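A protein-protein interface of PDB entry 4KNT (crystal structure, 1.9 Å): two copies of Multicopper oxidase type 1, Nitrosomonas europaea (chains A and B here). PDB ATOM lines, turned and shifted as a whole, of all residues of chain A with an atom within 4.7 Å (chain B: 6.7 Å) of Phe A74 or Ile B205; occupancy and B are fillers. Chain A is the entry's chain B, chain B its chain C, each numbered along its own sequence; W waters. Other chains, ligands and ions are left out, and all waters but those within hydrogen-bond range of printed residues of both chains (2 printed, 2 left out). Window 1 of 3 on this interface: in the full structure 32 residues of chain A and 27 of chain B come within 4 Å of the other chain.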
ATOM      1  N   SER A  60       3.182 -17.401   4.693  1.00  0.00           N
ATOM      2  CA  SER A  60       3.671 -16.606   5.809  1.00  0.00           C
ATOM      3  C   SER A  60       3.421 -17.340   7.120  1.00  0.00           C
ATOM      4  O   SER A  60       2.887 -18.455   7.131  1.00  0.00           O
ATOM      5  CB  SER A  60       2.998 -15.227   5.830  1.00  0.00           C
ATOM      6  OG  SER A  60       1.600 -15.346   6.016  1.00  0.00           O
ATOM      7  N   MET A  61       3.818 -16.716   8.223  1.00  0.00           N
ATOM      8  CA  MET A  61       3.547 -17.284   9.535  1.00  0.00           C
ATOM      9  C   MET A  61       3.089 -16.246  10.548  1.00  0.00           C
ATOM     10  O   MET A  61       3.726 -15.206  10.731  1.00  0.00           O
ATOM     11  CB  MET A  61       4.755 -18.048  10.072  1.00  0.00           C
ATOM     12  CG  MET A  61       4.559 -18.545  11.501  1.00  0.00           C
ATOM     13  SD  MET A  61       3.244 -19.766  11.647  1.00  0.00           S
ATOM     14  CE  MET A  61       4.169 -21.244  11.263  1.00  0.00           C
ATOM     15  N   ASP A  62       1.980 -16.568  11.210  1.00  0.00           N
ATOM     16  CA  ASP A  62       1.402 -15.760  12.271  1.00  0.00           C
ATOM     17  C   ASP A  62       1.290 -16.643  13.522  1.00  0.00           C
ATOM     18  O   ASP A  62       0.556 -17.627  13.512  1.00  0.00           O
ATOM     19  CB  ASP A  62       0.019 -15.270  11.805  1.00  0.00           C
ATOM     20  CG  ASP A  62      -0.743 -14.490  12.866  1.00  0.00           C
ATOM     21  OD1 ASP A  62      -0.547 -14.719  14.080  1.00  0.00           O
ATOM     22  OD2 ASP A  62      -1.578 -13.644  12.469  1.00  0.00           O
ATOM     23  N   PHE A  63       2.036 -16.300  14.578  1.00  0.00           N
ATOM     24  CA  PHE A  63       1.896 -16.944  15.893  1.00  0.00           C
ATOM     25  C   PHE A  63       1.064 -16.050  16.816  1.00  0.00           C
ATOM     26  O   PHE A  63       1.410 -14.882  17.009  1.00  0.00           O
ATOM     27  CB  PHE A  63       3.264 -17.153  16.564  1.00  0.00           C
ATOM     28  CG  PHE A  63       4.095 -18.270  15.984  1.00  0.00           C
ATOM     29  CD1 PHE A  63       3.887 -19.592  16.377  1.00  0.00           C
ATOM     30  CD2 PHE A  63       5.132 -17.992  15.098  1.00  0.00           C
ATOM     31  CE1 PHE A  63       4.670 -20.626  15.858  1.00  0.00           C
ATOM     32  CE2 PHE A  63       5.930 -19.017  14.579  1.00  0.00           C
ATOM     33  CZ  PHE A  63       5.697 -20.338  14.957  1.00  0.00           C
ATOM     34  N   ALA A  66       3.038 -14.438  19.676  1.00  0.00           N
ATOM     35  CA  ALA A  66       3.993 -13.377  19.357  1.00  0.00           C
ATOM     36  C   ALA A  66       3.363 -11.992  19.453  1.00  0.00           C
ATOM     37  O   ALA A  66       2.184 -11.808  19.138  1.00  0.00           O
ATOM     38  CB  ALA A  66       4.570 -13.595  17.968  1.00  0.00           C
ATOM     39  N   LEU A  68       4.310  -8.657  17.757  1.00  0.00           N
ATOM     40  CA  LEU A  68       5.194  -8.177  16.698  1.00  0.00           C
ATOM     41  C   LEU A  68       4.501  -7.143  15.800  1.00  0.00           C
ATOM     42  O   LEU A  68       3.511  -6.522  16.200  1.00  0.00           O
ATOM     43  CB  LEU A  68       5.709  -9.370  15.872  1.00  0.00           C
ATOM     44  CG  LEU A  68       6.620 -10.386  16.582  1.00  0.00           C
ATOM     45  CD1 LEU A  68       6.794 -11.659  15.764  1.00  0.00           C
ATOM     46  CD2 LEU A  68       7.983  -9.780  16.928  1.00  0.00           C
ATOM     47  N   ASP A  69       5.032  -6.959  14.593  1.00  0.00           N
ATOM     48  CA  ASP A  69       4.437  -6.058  13.605  1.00  0.00           C
ATOM     49  C   ASP A  69       3.825  -6.879  12.475  1.00  0.00           C
ATOM     50  O   ASP A  69       4.542  -7.573  11.753  1.00  0.00           O
ATOM     51  CB  ASP A  69       5.499  -5.078  13.081  1.00  0.00           C
ATOM     52  CG  ASP A  69       5.070  -4.344  11.811  1.00  0.00           C
ATOM     53  OD1 ASP A  69       3.853  -4.171  11.559  1.00  0.00           O
ATOM     54  OD2 ASP A  69       5.976  -3.921  11.065  1.00  0.00           O
ATOM     55  N   VAL A  70       2.504  -6.796  12.326  1.00  0.00           N
ATOM     56  CA  VAL A  70       1.792  -7.562  11.291  1.00  0.00           C
ATOM     57  C   VAL A  70       2.329  -7.315   9.874  1.00  0.00           C
ATOM     58  O   VAL A  70       2.398  -8.243   9.059  1.00  0.00           O
ATOM     59  CB  VAL A  70       0.246  -7.344  11.339  1.00  0.00           C
ATOM     60  CG1 VAL A  70      -0.132  -5.884  11.062  1.00  0.00           C
ATOM     61  CG2 VAL A  70      -0.470  -8.287  10.359  1.00  0.00           C
ATOM     62  N   GLU A  72       5.496  -6.241   8.736  1.00  0.00           N
ATOM     63  CA  GLU A  72       6.836  -6.724   8.405  1.00  0.00           C
ATOM     64  C   GLU A  72       7.087  -8.179   8.796  1.00  0.00           C
ATOM     65  O   GLU A  72       7.697  -8.932   8.038  1.00  0.00           O
ATOM     66  CB  GLU A  72       7.909  -5.821   9.020  1.00  0.00           C
ATOM     67  CG  GLU A  72       8.016  -4.441   8.368  1.00  0.00           C
ATOM     68  CD  GLU A  72       8.389  -4.504   6.895  1.00  0.00           C
ATOM     69  OE1 GLU A  72       9.238  -5.344   6.522  1.00  0.00           O
ATOM     70  OE2 GLU A  72       7.830  -3.706   6.105  1.00  0.00           O
ATOM     71  N   ASP A  73       6.622  -8.575   9.976  1.00  0.00           N
ATOM     72  CA  ASP A  73       6.939  -9.902  10.495  1.00  0.00           C
ATOM     73  C   ASP A  73       6.076 -10.999   9.886  1.00  0.00           C
ATOM     74  O   ASP A  73       6.590 -12.053   9.523  1.00  0.00           O
ATOM     75  CB  ASP A  73       6.868  -9.916  12.018  1.00  0.00           C
ATOM     76  CG  ASP A  73       7.878  -8.980  12.647  1.00  0.00           C
ATOM     77  OD1 ASP A  73       9.083  -9.126  12.353  1.00  0.00           O
ATOM     78  OD2 ASP A  73       7.464  -8.094  13.421  1.00  0.00           O
ATOM     79  N   PHE A  74       4.775 -10.742   9.764  1.00  0.00           N
ATOM     80  CA  PHE A  74       3.845 -11.726   9.203  1.00  0.00           C
ATOM     81  C   PHE A  74       3.690 -11.596   7.677  1.00  0.00           C
ATOM     82  O   PHE A  74       2.714 -12.085   7.103  1.00  0.00           O
ATOM     83  CB  PHE A  74       2.472 -11.655   9.899  1.00  0.00           C
ATOM     84  CG  PHE A  74       2.506 -11.929  11.393  1.00  0.00           C
ATOM     85  CD1 PHE A  74       3.651 -12.434  12.019  1.00  0.00           C
ATOM     86  CD2 PHE A  74       1.370 -11.709  12.167  1.00  0.00           C
ATOM     87  CE1 PHE A  74       3.669 -12.688  13.390  1.00  0.00           C
ATOM     88  CE2 PHE A  74       1.376 -11.964  13.541  1.00  0.00           C
ATOM     89  CZ  PHE A  74       2.526 -12.451  14.156  1.00  0.00           C
ATOM     90  N   GLU A  75       4.658 -10.953   7.025  1.00  0.00           N
ATOM     91  CA  GLU A  75       4.623 -10.760   5.565  1.00  0.00           C
ATOM     92  C   GLU A  75       4.689 -12.075   4.778  1.00  0.00           C
ATOM     93  O   GLU A  75       5.290 -13.052   5.231  1.00  0.00           O
ATOM     94  CB  GLU A  75       5.753  -9.825   5.115  1.00  0.00           C
ATOM     95  CG  GLU A  75       7.156 -10.442   5.198  1.00  0.00           C
ATOM     96  CD  GLU A  75       8.252  -9.500   4.730  1.00  0.00           C
ATOM     97  OE1 GLU A  75       7.941  -8.492   4.060  1.00  0.00           O
ATOM     98  OE2 GLU A  75       9.431  -9.770   5.039  1.00  0.00           O
ATOM     99  N   SER A  76       4.067 -12.086   3.600  1.00  0.00           N
ATOM    100  CA  SER A  76       4.111 -13.247   2.706  1.00  0.00           C
ATOM    101  C   SER A  76       5.445 -13.333   1.970  1.00  0.00           C
ATOM    102  O   SER A  76       6.012 -12.313   1.570  1.00  0.00           O
ATOM    103  CB  SER A  76       2.973 -13.188   1.684  1.00  0.00           C
ATOM    104  OG  SER A  76       1.715 -13.158   2.325  1.00  0.00           O
ATOM    105  N   TYR A  85      12.206 -14.367  11.719  1.00  0.00           N
ATOM    106  CA  TYR A  85      11.914 -13.402  12.775  1.00  0.00           C
ATOM    107  C   TYR A  85      12.028 -14.005  14.167  1.00  0.00           C
ATOM    108  O   TYR A  85      11.925 -15.222  14.340  1.00  0.00           O
ATOM    109  CB  TYR A  85      10.573 -12.670  12.568  1.00  0.00           C
ATOM    110  CG  TYR A  85       9.296 -13.495  12.638  1.00  0.00           C
ATOM    111  CD1 TYR A  85       8.820 -13.999  13.851  1.00  0.00           C
ATOM    112  CD2 TYR A  85       8.531 -13.715  11.493  1.00  0.00           C
ATOM    113  CE1 TYR A  85       7.626 -14.733  13.915  1.00  0.00           C
ATOM    114  CE2 TYR A  85       7.337 -14.442  11.544  1.00  0.00           C
ATOM    115  CZ  TYR A  85       6.893 -14.946  12.757  1.00  0.00           C
ATOM    116  OH  TYR A  85       5.715 -15.657  12.806  1.00  0.00           O
ATOM    117  N   MET A 104      -6.466 -15.247   4.033  1.00  0.00           N
ATOM    118  CA  MET A 104      -6.255 -16.121   5.193  1.00  0.00           C
ATOM    119  C   MET A 104      -7.283 -17.242   5.311  1.00  0.00           C
ATOM    120  O   MET A 104      -6.945 -18.352   5.729  1.00  0.00           O
ATOM    121  CB  MET A 104      -6.221 -15.317   6.493  1.00  0.00           C
ATOM    122  CG  MET A 104      -4.870 -14.736   6.814  1.00  0.00           C
ATOM    123  SD  MET A 104      -4.830 -13.925   8.426  1.00  0.00           S
ATOM    124  CE  MET A 104      -5.549 -12.334   8.021  1.00  0.00           C
ATOM    125  N   HIS B 203      -9.723 -10.459  17.784  1.00  0.00           N
ATOM    126  CA  HIS B 203      -8.311 -10.799  17.930  1.00  0.00           C
ATOM    127  C   HIS B 203      -7.441  -9.682  17.354  1.00  0.00           C
ATOM    128  O   HIS B 203      -7.727  -9.170  16.268  1.00  0.00           O
ATOM    129  CB  HIS B 203      -8.009 -12.116  17.197  1.00  0.00           C
ATOM    130  CG  HIS B 203      -6.549 -12.398  17.017  1.00  0.00           C
ATOM    131  ND1 HIS B 203      -5.736 -12.810  18.052  1.00  0.00           N
ATOM    132  CD2 HIS B 203      -5.757 -12.339  15.920  1.00  0.00           C
ATOM    133  CE1 HIS B 203      -4.506 -12.985  17.602  1.00  0.00           C
ATOM    134  NE2 HIS B 203      -4.491 -12.704  16.312  1.00  0.00           N
ATOM    135  N   PRO B 204      -6.374  -9.296  18.078  1.00  0.00           N
ATOM    136  CA  PRO B 204      -5.432  -8.355  17.491  1.00  0.00           C
ATOM    137  C   PRO B 204      -4.280  -9.100  16.809  1.00  0.00           C
ATOM    138  O   PRO B 204      -3.428  -9.678  17.490  1.00  0.00           O
ATOM    139  CB  PRO B 204      -4.940  -7.555  18.706  1.00  0.00           C
ATOM    140  CG  PRO B 204      -5.183  -8.459  19.914  1.00  0.00           C
ATOM    141  CD  PRO B 204      -6.000  -9.652  19.458  1.00  0.00           C
ATOM    142  N   ILE B 205      -4.265  -9.104  15.477  1.00  0.00           N
ATOM    143  CA  ILE B 205      -3.179  -9.752  14.732  1.00  0.00           C
ATOM    144  C   ILE B 205      -1.831  -9.130  15.107  1.00  0.00           C
ATOM    145  O   ILE B 205      -1.678  -7.910  15.063  1.00  0.00           O
ATOM    146  CB  ILE B 205      -3.383  -9.702  13.197  1.00  0.00           C
ATOM    147  CG1 ILE B 205      -4.730 -10.322  12.808  1.00  0.00           C
ATOM    148  CG2 ILE B 205      -2.239 -10.437  12.487  1.00  0.00           C
ATOM    149  CD1 ILE B 205      -5.035 -10.272  11.311  1.00  0.00           C
ATOM    150  N   ALA B 206      -0.882  -9.989  15.492  1.00  0.00           N
ATOM    151  CA  ALA B 206       0.469  -9.608  15.940  1.00  0.00           C
ATOM    152  C   ALA B 206       0.489  -9.055  17.364  1.00  0.00           C
ATOM    153  O   ALA B 206       1.490  -8.485  17.807  1.00  0.00           O
ATOM    154  CB  ALA B 206       1.143  -8.638  14.956  1.00  0.00           C
ATOM    155  N   GLY B 207      -0.618  -9.239  18.079  1.00  0.00           N
ATOM    156  CA  GLY B 207      -0.725  -8.802  19.463  1.00  0.00           C
ATOM    157  C   GLY B 207      -1.509  -9.773  20.324  1.00  0.00           C
ATOM    158  O   GLY B 207      -1.808 -10.898  19.910  1.00  0.00           O
ATOM    159  N   ILE B 208      -1.831  -9.325  21.533  1.00  0.00           N
ATOM    160  CA  ILE B 208      -2.638 -10.086  22.481  1.00  0.00           C
ATOM    161  C   ILE B 208      -3.416  -9.088  23.332  1.00  0.00           C
ATOM    162  O   ILE B 208      -2.945  -7.976  23.576  1.00  0.00           O
ATOM    163  CB  ILE B 208      -1.755 -11.029  23.367  1.00  0.00           C
ATOM    164  CG1 ILE B 208      -2.614 -12.061  24.114  1.00  0.00           C
ATOM    165  CG2 ILE B 208      -0.857 -10.227  24.334  1.00  0.00           C
ATOM    166  CD1 ILE B 208      -1.822 -13.221  24.710  1.00  0.00           C
ATOM    167  N   ALA B 247       2.445  -2.373  13.376  1.00  0.00           N
ATOM    168  CA  ALA B 247       0.989  -2.425  13.360  1.00  0.00           C
ATOM    169  C   ALA B 247       0.435  -3.712  13.950  1.00  0.00           C
ATOM    170  O   ALA B 247       1.091  -4.758  13.919  1.00  0.00           O
ATOM    171  CB  ALA B 247       0.464  -2.228  11.940  1.00  0.00           C
ATOM    172  N   ASN B 248      -0.763  -3.602  14.517  1.00  0.00           N
ATOM    173  CA  ASN B 248      -1.632  -4.742  14.770  1.00  0.00           C
ATOM    174  C   ASN B 248      -2.898  -4.562  13.940  1.00  0.00           C
ATOM    175  O   ASN B 248      -3.263  -3.432  13.591  1.00  0.00           O
ATOM    176  CB  ASN B 248      -2.001  -4.853  16.253  1.00  0.00           C
ATOM    177  CG  ASN B 248      -0.850  -5.351  17.121  1.00  0.00           C
ATOM    178  OD1 ASN B 248       0.276  -5.545  16.656  1.00  0.00           O
ATOM    179  ND2 ASN B 248      -1.136  -5.559  18.393  1.00  0.00           N
ATOM    180  N   ALA B 249      -3.555  -5.667  13.606  1.00  0.00           N
ATOM    181  CA  ALA B 249      -4.835  -5.601  12.919  1.00  0.00           C
ATOM    182  C   ALA B 249      -5.911  -6.244  13.783  1.00  0.00           C
ATOM    183  O   ALA B 249      -5.914  -7.461  13.980  1.00  0.00           O
ATOM    184  CB  ALA B 249      -4.754  -6.274  11.546  1.00  0.00           C
ATOM    185  N   ILE B 250      -6.805  -5.417  14.319  1.00  0.00           N
ATOM    186  CA  ILE B 250      -7.938  -5.903  15.109  1.00  0.00           C
ATOM    187  C   ILE B 250      -8.968  -6.505  14.156  1.00  0.00           C
ATOM    188  O   ILE B 250      -9.509  -5.809  13.295  1.00  0.00           O
ATOM    189  CB  ILE B 250      -8.565  -4.781  15.979  1.00  0.00           C
ATOM    190  CG1 ILE B 250      -7.519  -4.223  16.956  1.00  0.00           C
ATOM    191  CG2 ILE B 250      -9.803  -5.301  16.730  1.00  0.00           C
ATOM    192  CD1 ILE B 250      -7.895  -2.895  17.596  1.00  0.00           C
ATOM    193  N   VAL B 251      -9.208  -7.805  14.295  1.00  0.00           N
ATOM    194  CA  VAL B 251     -10.094  -8.521  13.381  1.00  0.00           C
ATOM    195  C   VAL B 251     -11.160  -9.337  14.104  1.00  0.00           C
ATOM    196  O   VAL B 251     -10.972  -9.760  15.247  1.00  0.00           O
ATOM    197  CB  VAL B 251      -9.310  -9.466  12.405  1.00  0.00           C
ATOM    198  CG1 VAL B 251      -8.306  -8.687  11.580  1.00  0.00           C
ATOM    199  CG2 VAL B 251      -8.615 -10.616  13.161  1.00  0.00           C
ATOM    200  N   HIS B 253     -12.110 -12.775  13.982  1.00  0.00           N
ATOM    201  CA  HIS B 253     -11.313 -13.914  13.496  1.00  0.00           C
ATOM    202  C   HIS B 253     -12.122 -14.997  12.767  1.00  0.00           C
ATOM    203  O   HIS B 253     -11.540 -15.952  12.229  1.00  0.00           O
ATOM    204  CB  HIS B 253     -10.425 -14.507  14.600  1.00  0.00           C
ATOM    205  CG  HIS B 253      -9.133 -15.081  14.090  1.00  0.00           C
ATOM    206  ND1 HIS B 253      -9.082 -16.148  13.218  1.00  0.00           N
ATOM    207  CD2 HIS B 253      -7.846 -14.735  14.332  1.00  0.00           C
ATOM    208  CE1 HIS B 253      -7.822 -16.435  12.945  1.00  0.00           C
ATOM    209  NE2 HIS B 253      -7.052 -15.593  13.608  1.00  0.00           N
ATOM    210  N   MET B 255     -13.044 -15.708   9.759  1.00  0.00           N
ATOM    211  CA  MET B 255     -12.429 -15.119   8.560  1.00  0.00           C
ATOM    212  C   MET B 255     -13.384 -14.553   7.512  1.00  0.00           C
ATOM    213  O   MET B 255     -13.056 -13.563   6.859  1.00  0.00           O
ATOM    214  CB  MET B 255     -11.419 -16.074   7.910  1.00  0.00           C
ATOM    215  CG  MET B 255     -10.057 -16.155   8.614  1.00  0.00           C
ATOM    216  SD  MET B 255      -9.321 -14.592   9.175  1.00  0.00           S
ATOM    217  CE  MET B 255      -9.112 -13.675   7.665  1.00  0.00           C
ATOM    218  N   ILE B 263     -11.931  -5.531   9.725  1.00  0.00           N
ATOM    219  CA  ILE B 263     -10.512  -5.390  10.061  1.00  0.00           C
ATOM    220  C   ILE B 263     -10.227  -3.915  10.346  1.00  0.00           C
ATOM    221  O   ILE B 263     -10.544  -3.051   9.526  1.00  0.00           O
ATOM    222  CB  ILE B 263      -9.573  -5.877   8.910  1.00  0.00           C
ATOM    223  CG1 ILE B 263      -9.851  -7.342   8.546  1.00  0.00           C
ATOM    224  CG2 ILE B 263      -8.097  -5.684   9.301  1.00  0.00           C
ATOM    225  CD1 ILE B 263      -9.049  -7.875   7.346  1.00  0.00           C
HETATM  226  O   HOH W   1      -1.542 -12.764  15.674  1.00  0.00           O
HETATM  227  O   HOH W   2       3.106  -5.727  18.813  1.00  0.00           O
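The backbone NH (N) of Leu A68 is in hydrogen-bond range of the backbone carbonyl oxygen (O) of Ala B206, at 2.8 Å. The side-chain amide oxygen (OD1) of Asn B248 lies close to the backbone carbonyl oxygen (O) of Leu A68. The backbone NH (N) of Ala B247 lies within hydrogen-bond range of the side-chain carboxylate (OD1) of Asp A69 (2.9 Å). The backbone carbonyl oxygen of Ala B247 sits at hydrogen-bond distance from the backbone NH of Val A70 (2.9 Å).
The side-chain carboxylate of Asp A69 is in hydrogen-bond range of the backbone NH of Glu A72. The side-chain carboxylate of Asp A73 sits at hydrogen-bond distance from the backbone NH of Asp A69. The backbone carbonyl oxygen (O) of Ile B205 lies close to the side-chain amide oxygen (OD1) of Asn B248 (3.5 Å). The backbone carbonyl oxygen of Ala B249 sits at hydrogen-bond distance from the backbone NH of Ile B205 (2.8 Å). The side-chain amide oxygen of Asn B248 lies close to the backbone carbonyl oxygen of Ala B206.
Among the printed residues, pairs that only touch across the chains: Asp A62 with Ile B205, Ala A66 with Ala B206, Ala A66 with Gly B207, Leu A68 with Ala B247, Val A70 with Ile B205, Val A70 with Ala B206, Phe A74 with Ile B205, Phe A74 with Ala B206, Met A104 with Ile B205 and Met A104 with Met B255.
Met A61 touches none of the printed residues of chain B. Printed residues of chain B within 4 Å of Ala A66: Ala B206 (3.6 Å) and Gly B207 (3.9 Å). Of the printed residues of chain B, Leu A68 touches Ala B206, Ala B247 and Asn B248. Of the printed residues of chain B, Asp A69 touches Ala B247 (2.9 Å). Ile B205 touches just these residues of chain A: Asp A62, Val A70, Phe A74 and Met A104. The nearest residue of chain B that does not touch Phe A74 is Gly B207 (5.7 Å). The nearest printed residue of chain A that does not touch Ile B205 is Leu A68 (5.5 Å).
Printed residues of chain B that touch a printed residue of chain A: Ile B205, Ala B206, Gly B207, Ala B247, Asn B248 and Met B255. Hydrophobic or aromatic side chains of chain B within 4 Å of the printed part of chain A: Ile B205, Ala B206, Ala B247 and Met B255. Hydrophobic or aromatic side chains of chain A that line the printed part of chain B: Val A70, Phe A74 and Met A104. Among the printed residues, 14 pairs touch across the chains. Among the printed residues, no Asp or Glu carboxylate lies within 4 Å of a Lys or Arg side-chain nitrogen of the other chain.
No position is printed for both chains. Of the 14 pairs that touch across the chains among the printed residues, none has its exchanged pair printed and touching as well.
Water W1 lies within hydrogen-bond range of the side-chain carboxylate of Asp A62 (2.7 Å), the backbone NH of Ala B206 (2.9 Å) and a ring nitrogen (NE2) of His B203 (3.0 Å). Water W2 lies within hydrogen-bond range of O of Leu A68 and O of Ala B206.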
